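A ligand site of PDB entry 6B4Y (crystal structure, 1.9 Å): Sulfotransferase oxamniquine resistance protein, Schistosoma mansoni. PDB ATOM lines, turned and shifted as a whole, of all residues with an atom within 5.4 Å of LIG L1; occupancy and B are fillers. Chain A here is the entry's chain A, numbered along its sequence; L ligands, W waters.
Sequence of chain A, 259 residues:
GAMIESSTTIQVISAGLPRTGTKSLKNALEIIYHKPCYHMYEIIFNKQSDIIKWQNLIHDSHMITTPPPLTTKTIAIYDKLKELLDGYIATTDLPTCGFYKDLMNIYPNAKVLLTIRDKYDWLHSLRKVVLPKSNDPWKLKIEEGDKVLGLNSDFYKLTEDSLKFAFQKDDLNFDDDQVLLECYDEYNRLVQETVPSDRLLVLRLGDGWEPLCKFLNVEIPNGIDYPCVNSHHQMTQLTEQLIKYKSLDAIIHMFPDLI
The side-chain hydroxyl (OG) of Ser 125 sits at hydrogen-bond distance from an oxygen (O2) of LIG L1, at 2.4 Å.
The backbone NH of Thr 22 is in hydrogen-bond range of an oxygen (O4) of LIG L1 (2.8 Å).
OG1 of Thr 22 is in hydrogen-bond range of O4 of LIG L1, at 2.7 Å.
OG of Ser 24 sits at hydrogen-bond distance from N2 of LIG L1.
The guanidinium group (NH2) of Arg 117 is in salt-bridge range of an oxygen (O1) of LIG L1 (2.8 Å).
O4 of LIG L1 sits at hydrogen-bond distance from N of Arg 19, 2.8 Å away.
The guanidinium group (NH1) of Arg 19 lies within salt-bridge range of an oxygen (O6) of LIG L1 (2.9 Å).
The backbone NH (N) of Gly 21 lies within hydrogen-bond range of an oxygen (O7) of LIG L1 (2.9 Å).
O5 of LIG L1 sits at hydrogen-bond distance from ND2 of Asn 230, at 2.9 Å.
The backbone NH of Lys 23 lies within hydrogen-bond range of an oxygen (O5) of LIG L1, at 3.0 Å.
An oxygen (O2) of LIG L1 is in hydrogen-bond range of the backbone NH of His 232, 3.0 Å away.
A nitrogen (N3) of LIG L1 lies within hydrogen-bond range of the backbone carbonyl oxygen (O) of Pro 227.
An oxygen (O4) of LIG L1 lies within hydrogen-bond range of the backbone NH (N) of Thr 20 (3.0 Å).
O3 of LG2 L2 sits at hydrogen-bond distance from OD2 of Asp 93, 2.4 Å away.
Water W4 lies within hydrogen-bond range of O5 of LIG L1 (2.8 Å), N of Ser 24 (2.9 Å), O of Val 229 (3.0 Å) and N of Lys 23 (3.4 Å).
Water W3 bridges an oxygen (O1) of LIG L1 and the backbone carbonyl oxygen of Asp 121.
Pro 18 touches LIG L1 (C to O4, 3.8 Å).
CD2 of Leu 205 touches C10 of LIG L1, at 3.4 Å.
CD1 of Tyr 226 touches N3 of LIG L1 (3.95 Å).
Cys 228 touches LIG L1 (CB to N3, 3.7 Å).
Val 229 touches LIG L1 (O to C6, 3.5 Å).
Ser 231 touches LIG L1.
Hydrophobic or aromatic side chains that line LIG L1: Leu 205, Tyr 226 and His 232.
The nearest printed residue that does not touch LIG L1 is Gly 206 (4.1 Å).
OG of Ser 125 lies within hydrogen-bond range of NE of Arg 19 (2.9 Å).
A ring nitrogen (NE2) of His 39 lies within hydrogen-bond range of the side-chain hydroxyl (OG1) of Thr 22 (3.0 Å).
OG of Ser 24 sits at hydrogen-bond distance from O of Pro 227.
The side-chain hydroxyl (OG) of Ser 24 sits at hydrogen-bond distance from the backbone NH (N) of Val 229.
The guanidinium group (NH1) of Arg 117 is in hydrogen-bond range of the backbone carbonyl oxygen (O) of Arg 19 (2.8 Å).
The backbone carbonyl oxygen (O) of Asn 230 lies within hydrogen-bond range of the guanidinium group (NH2) of Arg 19 (2.7 Å).
OG1 of Thr 20 sits at hydrogen-bond distance from O of Leu 17, 2.6 Å away.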
ATOM      1  N   LEU A  17      -8.179   3.569 -17.224  1.00  0.00           N
ATOM      2  CA  LEU A  17      -6.760   3.788 -17.441  1.00  0.00           C
ATOM      3  C   LEU A  17      -5.993   3.883 -16.139  1.00  0.00           C
ATOM      4  O   LEU A  17      -6.583   4.106 -15.077  1.00  0.00           O
ATOM      5  CB  LEU A  17      -6.574   5.060 -18.272  1.00  0.00           C
ATOM      6  CG  LEU A  17      -7.182   4.943 -19.664  1.00  0.00           C
ATOM      7  CD1 LEU A  17      -7.197   6.324 -20.328  1.00  0.00           C
ATOM      8  CD2 LEU A  17      -6.397   3.946 -20.476  1.00  0.00           C
ATOM      9  N   PRO A  18      -4.662   3.731 -16.188  1.00  0.00           N
ATOM     10  CA  PRO A  18      -3.864   3.927 -14.983  1.00  0.00           C
ATOM     11  C   PRO A  18      -4.044   5.339 -14.385  1.00  0.00           C
ATOM     12  O   PRO A  18      -4.316   6.271 -15.133  1.00  0.00           O
ATOM     13  CB  PRO A  18      -2.425   3.733 -15.472  1.00  0.00           C
ATOM     14  CG  PRO A  18      -2.508   3.750 -16.961  1.00  0.00           C
ATOM     15  CD  PRO A  18      -3.845   3.241 -17.316  1.00  0.00           C
ATOM     16  N   ARG A  19      -3.882   5.453 -13.062  1.00  0.00           N
ATOM     17  CA  ARG A  19      -4.026   6.690 -12.306  1.00  0.00           C
ATOM     18  C   ARG A  19      -5.474   7.189 -12.265  1.00  0.00           C
ATOM     19  O   ARG A  19      -5.713   8.387 -12.118  1.00  0.00           O
ATOM     20  CB  ARG A  19      -3.100   7.802 -12.862  1.00  0.00           C
ATOM     21  CG  ARG A  19      -1.636   7.356 -13.101  1.00  0.00           C
ATOM     22  CD  ARG A  19      -1.086   6.592 -11.882  1.00  0.00           C
ATOM     23  NE  ARG A  19      -1.042   7.448 -10.687  1.00  0.00           N
ATOM     24  CZ  ARG A  19      -0.731   7.004  -9.466  1.00  0.00           C
ATOM     25  NH1 ARG A  19      -0.482   5.717  -9.269  1.00  0.00           N
ATOM     26  NH2 ARG A  19      -0.688   7.836  -8.430  1.00  0.00           N
ATOM     27  N   THR A  20      -6.427   6.259 -12.346  1.00  0.00           N
ATOM     28  CA  THR A  20      -7.845   6.595 -12.173  1.00  0.00           C
ATOM     29  C   THR A  20      -8.477   5.834 -11.019  1.00  0.00           C
ATOM     30  O   THR A  20      -9.696   5.707 -10.952  1.00  0.00           O
ATOM     31  CB  THR A  20      -8.671   6.298 -13.441  1.00  0.00           C
ATOM     32  OG1 THR A  20      -8.683   4.883 -13.689  1.00  0.00           O
ATOM     33  CG2 THR A  20      -8.046   6.996 -14.646  1.00  0.00           C
ATOM     34  N   GLY A  21      -7.654   5.331 -10.109  1.00  0.00           N
ATOM     35  CA  GLY A  21      -8.143   4.602  -8.946  1.00  0.00           C
ATOM     36  C   GLY A  21      -8.208   3.100  -9.139  1.00  0.00           C
ATOM     37  O   GLY A  21      -8.995   2.420  -8.474  1.00  0.00           O
ATOM     38  N   THR A  22      -7.381   2.567 -10.028  1.00  0.00           N
ATOM     39  CA  THR A  22      -7.417   1.141 -10.331  1.00  0.00           C
ATOM     40  C   THR A  22      -6.896   0.291  -9.156  1.00  0.00           C
ATOM     41  O   THR A  22      -7.412  -0.774  -8.889  1.00  0.00           O
ATOM     42  CB  THR A  22      -6.602   0.830 -11.601  1.00  0.00           C
ATOM     43  OG1 THR A  22      -5.228   1.155 -11.367  1.00  0.00           O
ATOM     44  CG2 THR A  22      -7.108   1.663 -12.776  1.00  0.00           C
ATOM     45  N   LYS A  23      -5.903   0.789  -8.435  1.00  0.00           N
ATOM     46  CA  LYS A  23      -5.406   0.020  -7.295  1.00  0.00           C
ATOM     47  C   LYS A  23      -6.401  -0.036  -6.126  1.00  0.00           C
ATOM     48  O   LYS A  23      -6.523  -1.076  -5.489  1.00  0.00           O
ATOM     49  CB  LYS A  23      -4.057   0.563  -6.824  1.00  0.00           C
ATOM     50  CG  LYS A  23      -3.395  -0.304  -5.744  1.00  0.00           C
ATOM     51  CD  LYS A  23      -3.253  -1.748  -6.221  1.00  0.00           C
ATOM     52  CE  LYS A  23      -2.337  -2.581  -5.333  1.00  0.00           C
ATOM     53  NZ  LYS A  23      -2.663  -2.570  -3.887  1.00  0.00           N
ATOM     54  N   SER A  24      -7.086   1.079  -5.812  1.00  0.00           N
ATOM     55  CA  SER A  24      -8.164   1.021  -4.826  1.00  0.00           C
ATOM     56  C   SER A  24      -9.266   0.046  -5.241  1.00  0.00           C
ATOM     57  O   SER A  24      -9.794  -0.700  -4.418  1.00  0.00           O
ATOM     58  CB  SER A  24      -8.779   2.408  -4.586  1.00  0.00           C
ATOM     59  OG  SER A  24      -7.783   3.280  -4.098  1.00  0.00           O
ATOM     60  N   HIS A  39      -3.647  -6.601 -11.896  1.00  0.00           N
ATOM     61  CA  HIS A  39      -3.258  -5.192 -11.826  1.00  0.00           C
ATOM     62  C   HIS A  39      -1.789  -5.131 -12.247  1.00  0.00           C
ATOM     63  O   HIS A  39      -1.144  -6.150 -12.218  1.00  0.00           O
ATOM     64  CB  HIS A  39      -3.412  -4.645 -10.413  1.00  0.00           C
ATOM     65  CG  HIS A  39      -3.246  -3.161 -10.302  1.00  0.00           C
ATOM     66  ND1 HIS A  39      -2.018  -2.561 -10.101  1.00  0.00           N
ATOM     67  CD2 HIS A  39      -4.142  -2.162 -10.385  1.00  0.00           C
ATOM     68  CE1 HIS A  39      -2.173  -1.248 -10.049  1.00  0.00           C
ATOM     69  NE2 HIS A  39      -3.454  -0.985 -10.213  1.00  0.00           N
ATOM     70  N   ASP A  93      -6.375  -1.935 -14.846  1.00  0.00           N
ATOM     71  CA  ASP A  93      -5.093  -1.300 -15.169  1.00  0.00           C
ATOM     72  C   ASP A  93      -4.417  -1.884 -16.428  1.00  0.00           C
ATOM     73  O   ASP A  93      -4.870  -2.882 -16.992  1.00  0.00           O
ATOM     74  CB  ASP A  93      -4.168  -1.431 -13.950  1.00  0.00           C
ATOM     75  CG  ASP A  93      -2.973  -0.508 -13.998  1.00  0.00           C
ATOM     76  OD1 ASP A  93      -3.010   0.541 -14.677  1.00  0.00           O
ATOM     77  OD2 ASP A  93      -1.984  -0.834 -13.313  1.00  0.00           O
ATOM     78  N   ARG A 117     -11.704  10.293 -14.156  1.00  0.00           N
ATOM     79  CA  ARG A 117     -11.463  11.462 -13.312  1.00  0.00           C
ATOM     80  C   ARG A 117     -11.175  12.681 -14.197  1.00  0.00           C
ATOM     81  O   ARG A 117     -11.056  12.545 -15.416  1.00  0.00           O
ATOM     82  CB  ARG A 117     -10.294  11.226 -12.338  1.00  0.00           C
ATOM     83  CG  ARG A 117      -8.912  11.312 -12.986  1.00  0.00           C
ATOM     84  CD  ARG A 117      -7.779  10.798 -12.077  1.00  0.00           C
ATOM     85  NE  ARG A 117      -7.455  11.723 -10.985  1.00  0.00           N
ATOM     86  CZ  ARG A 117      -6.380  11.609 -10.189  1.00  0.00           C
ATOM     87  NH1 ARG A 117      -5.515  10.620 -10.368  1.00  0.00           N
ATOM     88  NH2 ARG A 117      -6.165  12.495  -9.222  1.00  0.00           N
ATOM     89  N   ASP A 121      -6.016  16.353 -13.749  1.00  0.00           N
ATOM     90  CA  ASP A 121      -5.536  15.614 -12.568  1.00  0.00           C
ATOM     91  C   ASP A 121      -4.883  14.303 -13.011  1.00  0.00           C
ATOM     92  O   ASP A 121      -3.865  13.898 -12.475  1.00  0.00           O
ATOM     93  CB  ASP A 121      -6.655  15.307 -11.586  1.00  0.00           C
ATOM     94  CG  ASP A 121      -7.119  16.532 -10.791  1.00  0.00           C
ATOM     95  OD1 ASP A 121      -6.371  17.542 -10.738  1.00  0.00           O
ATOM     96  OD2 ASP A 121      -8.234  16.479 -10.214  1.00  0.00           O
ATOM     97  N   SER A 125      -0.902  13.151 -12.458  1.00  0.00           N
ATOM     98  CA  SER A 125      -0.613  11.919 -11.743  1.00  0.00           C
ATOM     99  C   SER A 125       0.230  10.966 -12.584  1.00  0.00           C
ATOM    100  O   SER A 125       1.179  10.354 -12.104  1.00  0.00           O
ATOM    101  CB  SER A 125      -1.928  11.219 -11.350  1.00  0.00           C
ATOM    102  OG  SER A 125      -1.699  10.229 -10.366  1.00  0.00           O
ATOM    103  N   LEU A 205     -13.814   8.830  -9.476  1.00  0.00           N
ATOM    104  CA  LEU A 205     -12.999   8.802  -8.280  1.00  0.00           C
ATOM    105  C   LEU A 205     -13.737   9.426  -7.110  1.00  0.00           C
ATOM    106  O   LEU A 205     -14.225  10.550  -7.214  1.00  0.00           O
ATOM    107  CB  LEU A 205     -11.687   9.562  -8.506  1.00  0.00           C
ATOM    108  CG  LEU A 205     -10.397   8.815  -8.804  1.00  0.00           C
ATOM    109  CD1 LEU A 205      -9.266   9.810  -8.799  1.00  0.00           C
ATOM    110  CD2 LEU A 205     -10.173   7.686  -7.805  1.00  0.00           C
ATOM    111  N   GLY A 206     -13.822   8.704  -6.001  1.00  0.00           N
ATOM    112  CA  GLY A 206     -14.477   9.210  -4.820  1.00  0.00           C
ATOM    113  C   GLY A 206     -15.858   8.615  -4.609  1.00  0.00           C
ATOM    114  O   GLY A 206     -16.466   8.816  -3.564  1.00  0.00           O
ATOM    115  N   TYR A 226     -13.896   2.289   1.894  1.00  0.00           N
ATOM    116  CA  TYR A 226     -13.464   2.078   0.517  1.00  0.00           C
ATOM    117  C   TYR A 226     -12.010   2.479   0.388  1.00  0.00           C
ATOM    118  O   TYR A 226     -11.646   3.555   0.820  1.00  0.00           O
ATOM    119  CB  TYR A 226     -14.332   2.879  -0.456  1.00  0.00           C
ATOM    120  CG  TYR A 226     -14.026   2.512  -1.884  1.00  0.00           C
ATOM    121  CD1 TYR A 226     -13.024   3.176  -2.594  1.00  0.00           C
ATOM    122  CD2 TYR A 226     -14.699   1.474  -2.519  1.00  0.00           C
ATOM    123  CE1 TYR A 226     -12.720   2.826  -3.899  1.00  0.00           C
ATOM    124  CE2 TYR A 226     -14.413   1.114  -3.812  1.00  0.00           C
ATOM    125  CZ  TYR A 226     -13.413   1.793  -4.503  1.00  0.00           C
ATOM    126  OH  TYR A 226     -13.116   1.437  -5.809  1.00  0.00           O
ATOM    127  N   PRO A 227     -11.171   1.610  -0.218  1.00  0.00           N
ATOM    128  CA  PRO A 227      -9.724   1.898  -0.262  1.00  0.00           C
ATOM    129  C   PRO A 227      -9.364   3.246  -0.877  1.00  0.00           C
ATOM    130  O   PRO A 227      -9.989   3.672  -1.834  1.00  0.00           O
ATOM    131  CB  PRO A 227      -9.158   0.767  -1.144  1.00  0.00           C
ATOM    132  CG  PRO A 227     -10.157  -0.300  -1.095  1.00  0.00           C
ATOM    133  CD  PRO A 227     -11.501   0.335  -0.880  1.00  0.00           C
ATOM    134  N   CYS A 228      -8.331   3.877  -0.331  1.00  0.00           N
ATOM    135  CA  CYS A 228      -7.759   5.074  -0.918  1.00  0.00           C
ATOM    136  C   CYS A 228      -6.234   4.928  -0.882  1.00  0.00           C
ATOM    137  O   CYS A 228      -5.587   5.305   0.097  1.00  0.00           O
ATOM    138  CB  CYS A 228      -8.212   6.322  -0.161  1.00  0.00           C
ATOM    139  SG  CYS A 228      -7.509   7.857  -0.795  1.00  0.00           S
ATOM    140  N   VAL A 229      -5.659   4.343  -1.930  1.00  0.00           N
ATOM    141  CA  VAL A 229      -4.235   4.027  -1.957  1.00  0.00           C
ATOM    142  C   VAL A 229      -3.624   4.413  -3.296  1.00  0.00           C
ATOM    143  O   VAL A 229      -4.350   4.736  -4.217  1.00  0.00           O
ATOM    144  CB  VAL A 229      -3.973   2.528  -1.705  1.00  0.00           C
ATOM    145  CG1 VAL A 229      -4.369   2.155  -0.284  1.00  0.00           C
ATOM    146  CG2 VAL A 229      -4.724   1.635  -2.718  1.00  0.00           C
ATOM    147  N   ASN A 230      -2.289   4.398  -3.361  1.00  0.00           N
ATOM    148  CA  ASN A 230      -1.546   4.551  -4.619  1.00  0.00           C
ATOM    149  C   ASN A 230      -1.529   5.987  -5.151  1.00  0.00           C
ATOM    150  O   ASN A 230      -1.462   6.210  -6.356  1.00  0.00           O
ATOM    151  CB  ASN A 230      -2.127   3.605  -5.705  1.00  0.00           C
ATOM    152  CG  ASN A 230      -1.074   3.177  -6.710  1.00  0.00           C
ATOM    153  OD1 ASN A 230       0.105   3.143  -6.397  1.00  0.00           O
ATOM    154  ND2 ASN A 230      -1.496   2.859  -7.931  1.00  0.00           N
ATOM    155  N   SER A 231      -1.565   6.964  -4.242  1.00  0.00           N
ATOM    156  CA  SER A 231      -1.407   8.365  -4.614  1.00  0.00           C
ATOM    157  C   SER A 231       0.018   8.624  -5.066  1.00  0.00           C
ATOM    158  O   SER A 231       0.933   7.923  -4.675  1.00  0.00           O
ATOM    159  CB  SER A 231      -1.759   9.293  -3.443  1.00  0.00           C
ATOM    160  OG  SER A 231      -0.821   9.152  -2.381  1.00  0.00           O
ATOM    161  N   HIS A 232       0.205   9.657  -5.884  1.00  0.00           N
ATOM    162  CA  HIS A 232       1.560   9.928  -6.379  1.00  0.00           C
ATOM    163  C   HIS A 232       2.495  10.346  -5.244  1.00  0.00           C
ATOM    164  O   HIS A 232       3.702  10.109  -5.310  1.00  0.00           O
ATOM    165  CB  HIS A 232       1.535  10.973  -7.497  1.00  0.00           C
ATOM    166  CG  HIS A 232       1.187  12.357  -7.048  1.00  0.00           C
ATOM    167  ND1 HIS A 232       2.105  13.201  -6.472  1.00  0.00           N
ATOM    168  CD2 HIS A 232       0.027  13.061  -7.139  1.00  0.00           C
ATOM    169  CE1 HIS A 232       1.530  14.364  -6.213  1.00  0.00           C
ATOM    170  NE2 HIS A 232       0.271  14.299  -6.596  1.00  0.00           N
ATOM    171  N   HIS A 233       1.946  10.929  -4.182  1.00  0.00           N
ATOM    172  CA  HIS A 233       2.747  11.251  -2.998  1.00  0.00           C
ATOM    173  C   HIS A 233       3.286   9.991  -2.333  1.00  0.00           C
ATOM    174  O   HIS A 233       4.449   9.935  -1.946  1.00  0.00           O
ATOM    175  CB  HIS A 233       1.925  12.044  -1.976  1.00  0.00           C
ATOM    176  CG  HIS A 233       1.552  13.420  -2.427  1.00  0.00           C
ATOM    177  ND1 HIS A 233       2.485  14.391  -2.698  1.00  0.00           N
ATOM    178  CD2 HIS A 233       0.331  13.980  -2.649  1.00  0.00           C
ATOM    179  CE1 HIS A 233       1.868  15.501  -3.069  1.00  0.00           C
ATOM    180  NE2 HIS A 233       0.568  15.274  -3.049  1.00  0.00           N
HETATM  181  P1  LIG L   1      -3.149  10.978  -7.357  1.00  0.00           P
HETATM  182  O1  LIG L   1      -3.610  12.239  -8.033  1.00  0.00           O
HETATM  183  O2  LIG L   1      -1.828  10.499  -7.937  1.00  0.00           O
HETATM  184  O3  LIG L   1      -3.003  11.154  -5.886  1.00  0.00           O
HETATM  185  P2  LIG L   1      -4.247   4.229  -9.918  1.00  0.00           P
HETATM  186  O4  LIG L   1      -5.106   3.818 -11.093  1.00  0.00           O
HETATM  187  O5  LIG L   1      -4.272   3.270  -8.767  1.00  0.00           O
HETATM  188  O6  LIG L   1      -2.806   4.418 -10.339  1.00  0.00           O
HETATM  189  O7  LIG L   1      -4.852   5.611  -9.386  1.00  0.00           O
HETATM  190  C1  LIG L   1      -4.239   6.280  -8.280  1.00  0.00           C
HETATM  191  C2  LIG L   1      -4.898   7.622  -8.117  1.00  0.00           C
HETATM  192  O8  LIG L   1      -6.246   7.437  -7.629  1.00  0.00           O
HETATM  193  C3  LIG L   1      -4.211   8.534  -7.146  1.00  0.00           C
HETATM  194  O9  LIG L   1      -4.318   9.876  -7.620  1.00  0.00           O
HETATM  195  C4  LIG L   1      -4.988   8.377  -5.903  1.00  0.00           C
HETATM  196  O10 LIG L   1      -4.886   9.551  -5.133  1.00  0.00           O
HETATM  197  C5  LIG L   1      -6.370   8.264  -6.457  1.00  0.00           C
HETATM  198  N1  LIG L   1      -7.272   7.601  -5.603  1.00  0.00           N
HETATM  199  C6  LIG L   1      -7.236   6.307  -5.304  1.00  0.00           C
HETATM  200  N2  LIG L   1      -8.251   6.007  -4.496  1.00  0.00           N
HETATM  201  C7  LIG L   1      -8.960   7.147  -4.267  1.00  0.00           C
HETATM  202  C8  LIG L   1     -10.138   7.447  -3.516  1.00  0.00           C
HETATM  203  N3  LIG L   1     -10.786   6.431  -2.787  1.00  0.00           N
HETATM  204  N4  LIG L   1     -10.580   8.703  -3.512  1.00  0.00           N
HETATM  205  C9  LIG L   1      -9.972   9.667  -4.198  1.00  0.00           C
HETATM  206  N5  LIG L   1      -8.881   9.421  -4.921  1.00  0.00           N
HETATM  207  C10 LIG L   1      -8.340   8.180  -4.991  1.00  0.00           C
HETATM  208  C1  LG2 L   2       1.799   1.543 -11.948  1.00  0.00           C
HETATM  209  C2  LG2 L   2       1.742   1.485 -13.344  1.00  0.00           C
HETATM  210  C3  LG2 L   2       2.953   1.595 -14.046  1.00  0.00           C
HETATM  211  C4  LG2 L   2       4.161   1.779 -13.386  1.00  0.00           C
HETATM  212  C5  LG2 L   2       4.194   1.835 -11.996  1.00  0.00           C
HETATM  213  C6  LG2 L   2       3.004   1.713 -11.272  1.00  0.00           C
HETATM  214  C7  LG2 L   2       5.468   2.012  -9.883  1.00  0.00           C
HETATM  215  C8  LG2 L   2       4.311   1.181  -9.346  1.00  0.00           C
HETATM  216  C9  LG2 L   2       3.008   1.757  -9.880  1.00  0.00           C
HETATM  217  C10 LG2 L   2       0.493   1.311 -13.942  1.00  0.00           C
HETATM  218  C11 LG2 L   2       6.808   1.503  -9.351  1.00  0.00           C
HETATM  219  C12 LG2 L   2       7.715   3.411  -7.453  1.00  0.00           C
HETATM  220  C13 LG2 L   2       9.786   3.802  -8.836  1.00  0.00           C
HETATM  221  C14 LG2 L   2       8.647   2.804  -8.509  1.00  0.00           C
HETATM  222  N1  LG2 L   2       5.440   1.993 -11.359  1.00  0.00           N
HETATM  223  N2  LG2 L   2       3.002   1.558 -15.381  1.00  0.00           N
HETATM  224  N3  LG2 L   2       7.896   2.426  -9.722  1.00  0.00           N
HETATM  225  O1  LG2 L   2       4.048   2.246 -15.966  1.00  0.00           O
HETATM  226  O2  LG2 L   2       2.034   0.685 -16.231  1.00  0.00           O
HETATM  227  O3  LG2 L   2      -0.476   1.039 -12.928  1.00  0.00           O
HETATM  228  O   HOH W   1      -8.075  12.176  -5.495  1.00  0.00           O
HETATM  229  O   HOH W   2     -12.203   9.780  -1.625  1.00  0.00           O
HETATM  230  O   HOH W   3      -3.082  14.366  -9.753  1.00  0.00           O
HETATM  231  O   HOH W   4      -5.891   3.588  -6.533  1.00  0.00           O
